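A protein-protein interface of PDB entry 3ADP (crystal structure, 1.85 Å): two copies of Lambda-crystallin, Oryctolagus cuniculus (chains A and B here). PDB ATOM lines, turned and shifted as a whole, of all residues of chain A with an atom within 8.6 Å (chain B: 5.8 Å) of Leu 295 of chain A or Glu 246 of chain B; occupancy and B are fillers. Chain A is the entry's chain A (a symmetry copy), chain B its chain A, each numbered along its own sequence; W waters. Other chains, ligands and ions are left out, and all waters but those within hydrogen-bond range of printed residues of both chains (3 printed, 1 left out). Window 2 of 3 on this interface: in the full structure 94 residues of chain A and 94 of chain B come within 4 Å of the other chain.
NH2 of Arg 299 of chain A lies within salt-bridge range of OE1 of Glu 246 of chain B, at 3.2 Å.
O of Val 288 of chain A sits at hydrogen-bond distance from NE2 of His 242 of chain B (2.9 Å).
The backbone carbonyl oxygen of Ala 245 of chain B sits at hydrogen-bond distance from the guanidinium group of Arg 299 of chain A, 2.9 Å away.
The guanidinium group (NE) of Arg 299 of chain A sits at hydrogen-bond distance from the backbone carbonyl oxygen (O) of Leu 243 of chain B (2.8 Å).
N of Glu 246 of chain B is in hydrogen-bond range of OG of Ser 250 of chain B.
The backbone carbonyl oxygen (O) of Asn 281 of chain A sits at hydrogen-bond distance from the side-chain sulfur (SG) of Cys 285 of chain A, at 3.3 Å.
A ring nitrogen (ND1) of His 242 of chain B is in hydrogen-bond range of the backbone NH (N) of Met 248 of chain B.
N of Gly 247 of chain B lies within hydrogen-bond range of O of His 242 of chain B (3.1 Å).
The guanidinium group (NH2) of Arg 302 of chain A is in salt-bridge range of the side-chain carboxylate (OD1) of Asp 303 of chain A (2.9 Å).
Among the printed residues, pairs that only touch across the chains: Asn 281 of chain A with Met 248 of chain B, Asn 281 of chain A with Leu 249 of chain B, Met 284 of chain A with His 242 of chain B, Met 284 of chain A with Met 248 of chain B, Cys 285 of chain A with His 242 of chain B, Leu 295 of chain A with Glu 246 of chain B, Arg 298 of chain A with Leu 243 of chain B and Arg 302 of chain A with Asn 244 of chain B.
His 294 of chain A touches none of the printed residues of chain B.
Leu 295 of chain A touches just one residue of chain B: Glu 246.
Ala 297 of chain A touches none of the printed residues of chain B.
Printed residues of chain A within 4 Å of Asn 244 of chain B: Arg 302.
Of chain A, only Arg 299 (2.9 Å) comes within 4 Å of Ala 245 of chain B.
Glu 246 of chain B touches just these residues of chain A: Leu 295 and Arg 299.
No residue of chain A comes within 4 Å of Gly 247 of chain B.
Printed residues of chain A within 4 Å of Leu 249 of chain B: Asn 281 (3.5 Å).
The nearest printed residue of chain B that does not touch Leu 295 of chain A is His 242 of chain B (4.03 Å).
Of the 11 printed residues of chain B, 7 touch a printed residue of chain A.
Hydrophobic or aromatic side chains of chain B within 4 Å of the printed part of chain A: His 242, Leu 243, Met 248 and Leu 249.
Among the printed residues, Asp or Glu carboxylates within 4 Å of a Lys or Arg side-chain nitrogen of the other chain: Arg 299 of chain A with Glu 246 of chain B (3.2 Å).
No position is printed for both chains.
Of the 12 pairs that touch across the chains among the printed residues, none has its exchanged pair printed and touching as well.
Water W2 lies within hydrogen-bond range of NH1 of Arg 302 of chain A (2.8 Å) and OD1 of Asn 244 of chain B (3.0 Å).
Water W3 lies within hydrogen-bond range of the guanidinium group of Arg 302 of chain A and the backbone carbonyl oxygen of Leu 243 of chain B.
Water W1 bridges the backbone carbonyl oxygen of Glu 246 of chain B (2.9 Å) and the backbone carbonyl oxygen of Ala 290 of chain A (3.0 Å).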
ATOM      1  N   ASN A 281       9.219  -3.159  32.591  1.00  0.00           N
ATOM      2  CA  ASN A 281       9.981  -3.481  31.387  1.00  0.00           C
ATOM      3  C   ASN A 281       9.978  -2.330  30.383  1.00  0.00           C
ATOM      4  O   ASN A 281      11.003  -2.030  29.765  1.00  0.00           O
ATOM      5  CB  ASN A 281       9.424  -4.741  30.719  1.00  0.00           C
ATOM      6  CG  ASN A 281      10.260  -5.184  29.540  1.00  0.00           C
ATOM      7  OD1 ASN A 281      11.459  -5.438  29.677  1.00  0.00           O
ATOM      8  ND2 ASN A 281       9.636  -5.276  28.370  1.00  0.00           N
ATOM      9  N   MET A 284      12.337   0.306  31.574  1.00  0.00           N
ATOM     10  CA  MET A 284      13.709  -0.175  31.465  1.00  0.00           C
ATOM     11  C   MET A 284      14.185  -0.164  30.016  1.00  0.00           C
ATOM     12  O   MET A 284      15.327   0.198  29.735  1.00  0.00           O
ATOM     13  CB  MET A 284      13.830  -1.593  32.039  1.00  0.00           C
ATOM     14  CG  MET A 284      13.604  -1.690  33.547  1.00  0.00           C
ATOM     15  SD  MET A 284      14.781  -0.725  34.524  1.00  0.00           S
ATOM     16  CE  MET A 284      13.785   0.701  34.956  1.00  0.00           C
ATOM     17  N   CYS A 285      13.314  -0.564  29.095  1.00  0.00           N
ATOM     18  CA  CYS A 285      13.677  -0.584  27.681  1.00  0.00           C
ATOM     19  C   CYS A 285      13.815   0.821  27.109  1.00  0.00           C
ATOM     20  O   CYS A 285      14.528   1.032  26.124  1.00  0.00           O
ATOM     21  CB  CYS A 285      12.645  -1.373  26.874  1.00  0.00           C
ATOM     22  SG  CYS A 285      12.700  -3.149  27.163  1.00  0.00           S
ATOM     23  N   LYS A 287      15.152   3.281  28.705  1.00  0.00           N
ATOM     24  CA  LYS A 287      16.481   3.697  29.134  1.00  0.00           C
ATOM     25  C   LYS A 287      17.542   2.878  28.398  1.00  0.00           C
ATOM     26  O   LYS A 287      18.546   3.415  27.926  1.00  0.00           O
ATOM     27  CB  LYS A 287      16.632   3.490  30.647  1.00  0.00           C
ATOM     28  CG  LYS A 287      15.769   4.410  31.500  1.00  0.00           C
ATOM     29  CD  LYS A 287      15.580   3.863  32.915  1.00  0.00           C
ATOM     30  CE  LYS A 287      16.901   3.616  33.630  1.00  0.00           C
ATOM     31  NZ  LYS A 287      16.697   3.041  35.002  1.00  0.00           N
ATOM     32  N   VAL A 288      17.306   1.574  28.304  1.00  0.00           N
ATOM     33  CA  VAL A 288      18.232   0.666  27.637  1.00  0.00           C
ATOM     34  C   VAL A 288      17.474  -0.387  26.829  1.00  0.00           C
ATOM     35  O   VAL A 288      16.976  -1.367  27.388  1.00  0.00           O
ATOM     36  CB  VAL A 288      19.127  -0.065  28.661  1.00  0.00           C
ATOM     37  CG1 VAL A 288      20.056  -1.041  27.943  1.00  0.00           C
ATOM     38  CG2 VAL A 288      19.933   0.942  29.465  1.00  0.00           C
ATOM     39  N   PRO A 289      17.375  -0.192  25.503  1.00  0.00           N
ATOM     40  CA  PRO A 289      16.672  -1.141  24.635  1.00  0.00           C
ATOM     41  C   PRO A 289      17.114  -2.573  24.922  1.00  0.00           C
ATOM     42  O   PRO A 289      18.305  -2.842  25.088  1.00  0.00           O
ATOM     43  CB  PRO A 289      17.064  -0.676  23.238  1.00  0.00           C
ATOM     44  CG  PRO A 289      17.153   0.803  23.410  1.00  0.00           C
ATOM     45  CD  PRO A 289      17.914   0.932  24.717  1.00  0.00           C
ATOM     46  N   ALA A 290      16.149  -3.485  24.979  1.00  0.00           N
ATOM     47  CA  ALA A 290      16.439  -4.883  25.274  1.00  0.00           C
ATOM     48  C   ALA A 290      16.959  -5.687  24.087  1.00  0.00           C
ATOM     49  O   ALA A 290      16.386  -6.714  23.727  1.00  0.00           O
ATOM     50  CB  ALA A 290      15.206  -5.554  25.851  1.00  0.00           C
ATOM     51  N   ASP A 291      18.036  -5.215  23.473  1.00  0.00           N
ATOM     52  CA  ASP A 291      18.638  -5.932  22.358  1.00  0.00           C
ATOM     53  C   ASP A 291      20.103  -6.153  22.710  1.00  0.00           C
ATOM     54  O   ASP A 291      20.674  -5.410  23.506  1.00  0.00           O
ATOM     55  CB  ASP A 291      18.492  -5.149  21.048  1.00  0.00           C
ATOM     56  CG  ASP A 291      19.089  -3.761  21.120  1.00  0.00           C
ATOM     57  OD1 ASP A 291      20.329  -3.641  21.207  1.00  0.00           O
ATOM     58  OD2 ASP A 291      18.310  -2.788  21.086  1.00  0.00           O
ATOM     59  N   PRO A 292      20.725  -7.191  22.134  1.00  0.00           N
ATOM     60  CA  PRO A 292      22.130  -7.511  22.401  1.00  0.00           C
ATOM     61  C   PRO A 292      23.086  -6.319  22.421  1.00  0.00           C
ATOM     62  O   PRO A 292      23.900  -6.186  23.333  1.00  0.00           O
ATOM     63  CB  PRO A 292      22.468  -8.504  21.292  1.00  0.00           C
ATOM     64  CG  PRO A 292      21.169  -9.220  21.093  1.00  0.00           C
ATOM     65  CD  PRO A 292      20.175  -8.084  21.098  1.00  0.00           C
ATOM     66  N   GLU A 293      22.981  -5.456  21.416  1.00  0.00           N
ATOM     67  CA  GLU A 293      23.853  -4.290  21.301  1.00  0.00           C
ATOM     68  C   GLU A 293      23.742  -3.296  22.457  1.00  0.00           C
ATOM     69  O   GLU A 293      24.749  -2.943  23.076  1.00  0.00           O
ATOM     70  CB  GLU A 293      23.577  -3.568  19.976  1.00  0.00           C
ATOM     71  CG  GLU A 293      24.529  -2.423  19.670  1.00  0.00           C
ATOM     72  CD  GLU A 293      24.161  -1.681  18.395  1.00  0.00           C
ATOM     73  OE1 GLU A 293      24.168  -2.307  17.312  1.00  0.00           O
ATOM     74  OE2 GLU A 293      23.862  -0.470  18.478  1.00  0.00           O
ATOM     75  N   HIS A 294      22.527  -2.841  22.748  1.00  0.00           N
ATOM     76  CA  HIS A 294      22.325  -1.874  23.827  1.00  0.00           C
ATOM     77  C   HIS A 294      22.561  -2.434  25.223  1.00  0.00           C
ATOM     78  O   HIS A 294      23.033  -1.720  26.109  1.00  0.00           O
ATOM     79  CB  HIS A 294      20.924  -1.267  23.748  1.00  0.00           C
ATOM     80  CG  HIS A 294      20.713  -0.400  22.546  1.00  0.00           C
ATOM     81  ND1 HIS A 294      20.425  -0.913  21.300  1.00  0.00           N
ATOM     82  CD2 HIS A 294      20.798   0.942  22.391  1.00  0.00           C
ATOM     83  CE1 HIS A 294      20.341   0.078  20.428  1.00  0.00           C
ATOM     84  NE2 HIS A 294      20.563   1.214  21.065  1.00  0.00           N
ATOM     85  N   LEU A 295      22.228  -3.705  25.429  1.00  0.00           N
ATOM     86  CA  LEU A 295      22.435  -4.323  26.732  1.00  0.00           C
ATOM     87  C   LEU A 295      23.934  -4.470  26.992  1.00  0.00           C
ATOM     88  O   LEU A 295      24.424  -4.157  28.080  1.00  0.00           O
ATOM     89  CB  LEU A 295      21.749  -5.691  26.787  1.00  0.00           C
ATOM     90  CG  LEU A 295      20.216  -5.676  26.811  1.00  0.00           C
ATOM     91  CD1 LEU A 295      19.688  -7.099  26.702  1.00  0.00           C
ATOM     92  CD2 LEU A 295      19.725  -5.017  28.095  1.00  0.00           C
ATOM     93  N   ALA A 296      24.662  -4.932  25.981  1.00  0.00           N
ATOM     94  CA  ALA A 296      26.103  -5.104  26.112  1.00  0.00           C
ATOM     95  C   ALA A 296      26.776  -3.759  26.370  1.00  0.00           C
ATOM     96  O   ALA A 296      27.672  -3.650  27.205  1.00  0.00           O
ATOM     97  CB  ALA A 296      26.672  -5.741  24.848  1.00  0.00           C
ATOM     98  N   ALA A 297      26.338  -2.731  25.651  1.00  0.00           N
ATOM     99  CA  ALA A 297      26.911  -1.400  25.808  1.00  0.00           C
ATOM    100  C   ALA A 297      26.712  -0.876  27.225  1.00  0.00           C
ATOM    101  O   ALA A 297      27.626  -0.301  27.818  1.00  0.00           O
ATOM    102  CB  ALA A 297      26.284  -0.439  24.804  1.00  0.00           C
ATOM    103  N   ARG A 298      25.518  -1.081  27.770  1.00  0.00           N
ATOM    104  CA  ARG A 298      25.218  -0.611  29.118  1.00  0.00           C
ATOM    105  C   ARG A 298      26.001  -1.404  30.160  1.00  0.00           C
ATOM    106  O   ARG A 298      26.447  -0.845  31.165  1.00  0.00           O
ATOM    107  CB  ARG A 298      23.715  -0.712  29.387  1.00  0.00           C
ATOM    108  CG  ARG A 298      23.264  -0.107  30.714  1.00  0.00           C
ATOM    109  CD  ARG A 298      23.553   1.390  30.805  1.00  0.00           C
ATOM    110  NE  ARG A 298      22.917   1.967  31.986  1.00  0.00           N
ATOM    111  CZ  ARG A 298      23.096   3.213  32.417  1.00  0.00           C
ATOM    112  NH1 ARG A 298      23.903   4.044  31.767  1.00  0.00           N
ATOM    113  NH2 ARG A 298      22.466   3.627  33.508  1.00  0.00           N
ATOM    114  N   ARG A 299      26.168  -2.704  29.926  1.00  0.00           N
ATOM    115  CA  ARG A 299      26.922  -3.540  30.859  1.00  0.00           C
ATOM    116  C   ARG A 299      28.377  -3.096  30.854  1.00  0.00           C
ATOM    117  O   ARG A 299      29.043  -3.096  31.888  1.00  0.00           O
ATOM    118  CB  ARG A 299      26.853  -5.016  30.457  1.00  0.00           C
ATOM    119  CG  ARG A 299      25.475  -5.638  30.578  1.00  0.00           C
ATOM    120  CD  ARG A 299      25.533  -7.139  30.346  1.00  0.00           C
ATOM    121  NE  ARG A 299      24.194  -7.712  30.263  1.00  0.00           N
ATOM    122  CZ  ARG A 299      23.660  -8.207  29.151  1.00  0.00           C
ATOM    123  NH1 ARG A 299      24.355  -8.208  28.021  1.00  0.00           N
ATOM    124  NH2 ARG A 299      22.426  -8.687  29.166  1.00  0.00           N
ATOM    125  N   GLU A 300      28.867  -2.733  29.673  1.00  0.00           N
ATOM    126  CA  GLU A 300      30.243  -2.283  29.517  1.00  0.00           C
ATOM    127  C   GLU A 300      30.459  -1.012  30.332  1.00  0.00           C
ATOM    128  O   GLU A 300      31.485  -0.858  31.000  1.00  0.00           O
ATOM    129  CB  GLU A 300      30.540  -2.023  28.039  1.00  0.00           C
ATOM    130  CG  GLU A 300      31.905  -1.421  27.767  1.00  0.00           C
ATOM    131  CD  GLU A 300      32.129  -1.143  26.292  1.00  0.00           C
ATOM    132  OE1 GLU A 300      32.244  -2.113  25.513  1.00  0.00           O
ATOM    133  OE2 GLU A 300      32.182   0.046  25.912  1.00  0.00           O
ATOM    134  N   TRP A 301      29.486  -0.107  30.268  1.00  0.00           N
ATOM    135  CA  TRP A 301      29.551   1.147  31.011  1.00  0.00           C
ATOM    136  C   TRP A 301      29.537   0.823  32.499  1.00  0.00           C
ATOM    137  O   TRP A 301      30.361   1.327  33.266  1.00  0.00           O
ATOM    138  CB  TRP A 301      28.343   2.026  30.665  1.00  0.00           C
ATOM    139  CG  TRP A 301      28.255   3.297  31.459  1.00  0.00           C
ATOM    140  CD1 TRP A 301      28.918   4.469  31.218  1.00  0.00           C
ATOM    141  CD2 TRP A 301      27.467   3.516  32.635  1.00  0.00           C
ATOM    142  NE1 TRP A 301      28.586   5.405  32.171  1.00  0.00           N
ATOM    143  CE2 TRP A 301      27.697   4.846  33.052  1.00  0.00           C
ATOM    144  CE3 TRP A 301      26.586   2.716  33.376  1.00  0.00           C
ATOM    145  CZ2 TRP A 301      27.078   5.394  34.181  1.00  0.00           C
ATOM    146  CZ3 TRP A 301      25.970   3.263  34.500  1.00  0.00           C
ATOM    147  CH2 TRP A 301      26.221   4.589  34.889  1.00  0.00           C
ATOM    148  N   ARG A 302      28.590  -0.023  32.898  1.00  0.00           N
ATOM    149  CA  ARG A 302      28.454  -0.435  34.292  1.00  0.00           C
ATOM    150  C   ARG A 302      29.769  -0.993  34.825  1.00  0.00           C
ATOM    151  O   ARG A 302      30.233  -0.604  35.901  1.00  0.00           O
ATOM    152  CB  ARG A 302      27.363  -1.503  34.418  1.00  0.00           C
ATOM    153  CG  ARG A 302      27.190  -2.068  35.823  1.00  0.00           C
ATOM    154  CD  ARG A 302      26.506  -3.423  35.765  1.00  0.00           C
ATOM    155  NE  ARG A 302      27.347  -4.399  35.077  1.00  0.00           N
ATOM    156  CZ  ARG A 302      26.922  -5.569  34.610  1.00  0.00           C
ATOM    157  NH1 ARG A 302      25.651  -5.927  34.752  1.00  0.00           N
ATOM    158  NH2 ARG A 302      27.772  -6.378  33.992  1.00  0.00           N
ATOM    159  N   ASP A 303      30.365  -1.907  34.068  1.00  0.00           N
ATOM    160  CA  ASP A 303      31.623  -2.529  34.470  1.00  0.00           C
ATOM    161  C   ASP A 303      32.767  -1.527  34.593  1.00  0.00           C
ATOM    162  O   ASP A 303      33.616  -1.657  35.477  1.00  0.00           O
ATOM    163  CB  ASP A 303      31.993  -3.645  33.489  1.00  0.00           C
ATOM    164  CG  ASP A 303      31.066  -4.846  33.604  1.00  0.00           C
ATOM    165  OD1 ASP A 303      30.135  -4.811  34.439  1.00  0.00           O
ATOM    166  OD2 ASP A 303      31.266  -5.829  32.862  1.00  0.00           O
ATOM    167  N   HIS B 242      17.375  -5.778  34.859  1.00  0.00           N
ATOM    168  CA  HIS B 242      17.330  -5.605  33.412  1.00  0.00           C
ATOM    169  C   HIS B 242      18.635  -6.019  32.735  1.00  0.00           C
ATOM    170  O   HIS B 242      18.627  -6.627  31.661  1.00  0.00           O
ATOM    171  CB  HIS B 242      17.037  -4.135  33.104  1.00  0.00           C
ATOM    172  CG  HIS B 242      16.686  -3.865  31.675  1.00  0.00           C
ATOM    173  ND1 HIS B 242      15.588  -4.425  31.059  1.00  0.00           N
ATOM    174  CD2 HIS B 242      17.262  -3.055  30.755  1.00  0.00           C
ATOM    175  CE1 HIS B 242      15.499  -3.968  29.822  1.00  0.00           C
ATOM    176  NE2 HIS B 242      16.503  -3.134  29.613  1.00  0.00           N
ATOM    177  N   LEU B 243      19.755  -5.689  33.372  1.00  0.00           N
ATOM    178  CA  LEU B 243      21.076  -6.001  32.832  1.00  0.00           C
ATOM    179  C   LEU B 243      21.635  -7.367  33.234  1.00  0.00           C
ATOM    180  O   LEU B 243      22.507  -7.899  32.544  1.00  0.00           O
ATOM    181  CB  LEU B 243      22.078  -4.916  33.246  1.00  0.00           C
ATOM    182  CG  LEU B 243      21.765  -3.475  32.830  1.00  0.00           C
ATOM    183  CD1 LEU B 243      22.806  -2.539  33.426  1.00  0.00           C
ATOM    184  CD2 LEU B 243      21.748  -3.364  31.308  1.00  0.00           C
ATOM    185  N   ASN B 244      21.150  -7.929  34.338  1.00  0.00           N
ATOM    186  CA  ASN B 244      21.646  -9.227  34.791  1.00  0.00           C
ATOM    187  C   ASN B 244      20.980 -10.406  34.100  1.00  0.00           C
ATOM    188  O   ASN B 244      21.128 -11.556  34.514  1.00  0.00           O
ATOM    189  CB  ASN B 244      21.523  -9.354  36.311  1.00  0.00           C
ATOM    190  CG  ASN B 244      22.554  -8.513  37.044  1.00  0.00           C
ATOM    191  OD1 ASN B 244      23.641  -8.251  36.520  1.00  0.00           O
ATOM    192  ND2 ASN B 244      22.232  -8.099  38.263  1.00  0.00           N
ATOM    193  N   ALA B 245      20.251 -10.098  33.035  1.00  0.00           N
ATOM    194  CA  ALA B 245      19.579 -11.092  32.204  1.00  0.00           C
ATOM    195  C   ALA B 245      19.461 -10.391  30.860  1.00  0.00           C
ATOM    196  O   ALA B 245      20.049  -9.328  30.669  1.00  0.00           O
ATOM    197  CB  ALA B 245      18.195 -11.427  32.761  1.00  0.00           C
ATOM    198  N   GLU B 246      18.721 -10.968  29.923  1.00  0.00           N
ATOM    199  CA  GLU B 246      18.572 -10.323  28.629  1.00  0.00           C
ATOM    200  C   GLU B 246      17.357  -9.407  28.664  1.00  0.00           C
ATOM    201  O   GLU B 246      16.476  -9.493  27.811  1.00  0.00           O
ATOM    202  CB  GLU B 246      18.418 -11.367  27.520  1.00  0.00           C
ATOM    203  CG  GLU B 246      19.635 -12.259  27.346  1.00  0.00           C
ATOM    204  CD  GLU B 246      20.941 -11.483  27.392  1.00  0.00           C
ATOM    205  OE1 GLU B 246      21.000 -10.372  26.826  1.00  0.00           O
ATOM    206  OE2 GLU B 246      21.913 -11.990  27.988  1.00  0.00           O
ATOM    207  N   GLY B 247      17.321  -8.529  29.663  1.00  0.00           N
ATOM    208  CA  GLY B 247      16.201  -7.615  29.803  1.00  0.00           C
ATOM    209  C   GLY B 247      15.317  -8.005  30.973  1.00  0.00           C
ATOM    210  O   GLY B 247      15.412  -9.120  31.485  1.00  0.00           O
ATOM    211  N   MET B 248      14.447  -7.092  31.394  1.00  0.00           N
ATOM    212  CA  MET B 248      13.550  -7.338  32.524  1.00  0.00           C
ATOM    213  C   MET B 248      12.670  -8.583  32.369  1.00  0.00           C
ATOM    214  O   MET B 248      12.501  -9.351  33.319  1.00  0.00           O
ATOM    215  CB  MET B 248      12.666  -6.109  32.757  1.00  0.00           C
ATOM    216  CG  MET B 248      11.671  -6.248  33.907  1.00  0.00           C
ATOM    217  SD  MET B 248      12.454  -6.536  35.518  1.00  0.00           S
ATOM    218  CE  MET B 248      13.523  -5.077  35.631  1.00  0.00           C
ATOM    219  N   LEU B 249      12.101  -8.781  31.182  1.00  0.00           N
ATOM    220  CA  LEU B 249      11.246  -9.939  30.950  1.00  0.00           C
ATOM    221  C   LEU B 249      12.047 -11.214  31.183  1.00  0.00           C
ATOM    222  O   LEU B 249      11.592 -12.127  31.868  1.00  0.00           O
ATOM    223  CB  LEU B 249      10.695  -9.925  29.521  1.00  0.00           C
ATOM    224  CG  LEU B 249       9.907  -8.673  29.124  1.00  0.00           C
ATOM    225  CD1 LEU B 249       9.439  -8.798  27.682  1.00  0.00           C
ATOM    226  CD2 LEU B 249       8.718  -8.482  30.067  1.00  0.00           C
ATOM    227  N   SER B 250      13.246 -11.256  30.611  1.00  0.00           N
ATOM    228  CA  SER B 250      14.138 -12.402  30.745  1.00  0.00           C
ATOM    229  C   SER B 250      14.483 -12.670  32.208  1.00  0.00           C
ATOM    230  O   SER B 250      14.503 -13.821  32.651  1.00  0.00           O
ATOM    231  CB  SER B 250      15.423 -12.154  29.947  1.00  0.00           C
ATOM    232  OG  SER B 250      16.389 -13.162  30.187  1.00  0.00           O
ATOM    233  N   TYR B 251      14.756 -11.606  32.959  1.00  0.00           N
ATOM    234  CA  TYR B 251      15.110 -11.757  34.379  1.00  0.00           C
ATOM    235  C   TYR B 251      13.962 -12.387  35.180  1.00  0.00           C
ATOM    236  O   TYR B 251      14.142 -13.276  36.000  1.00  0.00           O
ATOM    237  CB  TYR B 251      15.492 -10.391  34.987  1.00  0.00           C
ATOM    238  CG  TYR B 251      16.091 -10.555  36.356  1.00  0.00           C
ATOM    239  CD1 TYR B 251      15.264 -10.749  37.460  1.00  0.00           C
ATOM    240  CD2 TYR B 251      17.476 -10.477  36.542  1.00  0.00           C
ATOM    241  CE1 TYR B 251      15.810 -10.896  38.733  1.00  0.00           C
ATOM    242  CE2 TYR B 251      18.024 -10.614  37.816  1.00  0.00           C
ATOM    243  CZ  TYR B 251      17.199 -10.825  38.909  1.00  0.00           C
ATOM    244  OH  TYR B 251      17.739 -10.987  40.176  1.00  0.00           O
ATOM    245  N   ARG B 254      13.502 -16.058  34.264  1.00  0.00           N
ATOM    246  CA  ARG B 254      14.539 -16.887  34.859  1.00  0.00           C
ATOM    247  C   ARG B 254      14.566 -16.939  36.380  1.00  0.00           C
ATOM    248  O   ARG B 254      14.834 -17.991  36.957  1.00  0.00           O
ATOM    249  CB  ARG B 254      15.921 -16.423  34.389  1.00  0.00           C
ATOM    250  CG  ARG B 254      16.164 -16.519  32.895  1.00  0.00           C
ATOM    251  CD  ARG B 254      17.543 -15.975  32.532  1.00  0.00           C
ATOM    252  NE  ARG B 254      17.762 -15.965  31.089  1.00  0.00           N
ATOM    253  CZ  ARG B 254      18.829 -15.440  30.496  1.00  0.00           C
ATOM    254  NH1 ARG B 254      19.786 -14.879  31.223  1.00  0.00           N
ATOM    255  NH2 ARG B 254      18.934 -15.468  29.173  1.00  0.00           N
HETATM  256  O   HOH W   1      16.049  -9.426  24.921  1.00  0.00           O
HETATM  257  O   HOH W   2      23.525  -5.233  36.493  1.00  0.00           O
HETATM  258  O   HOH W   3      25.559  -8.571  33.513  1.00  0.00           O
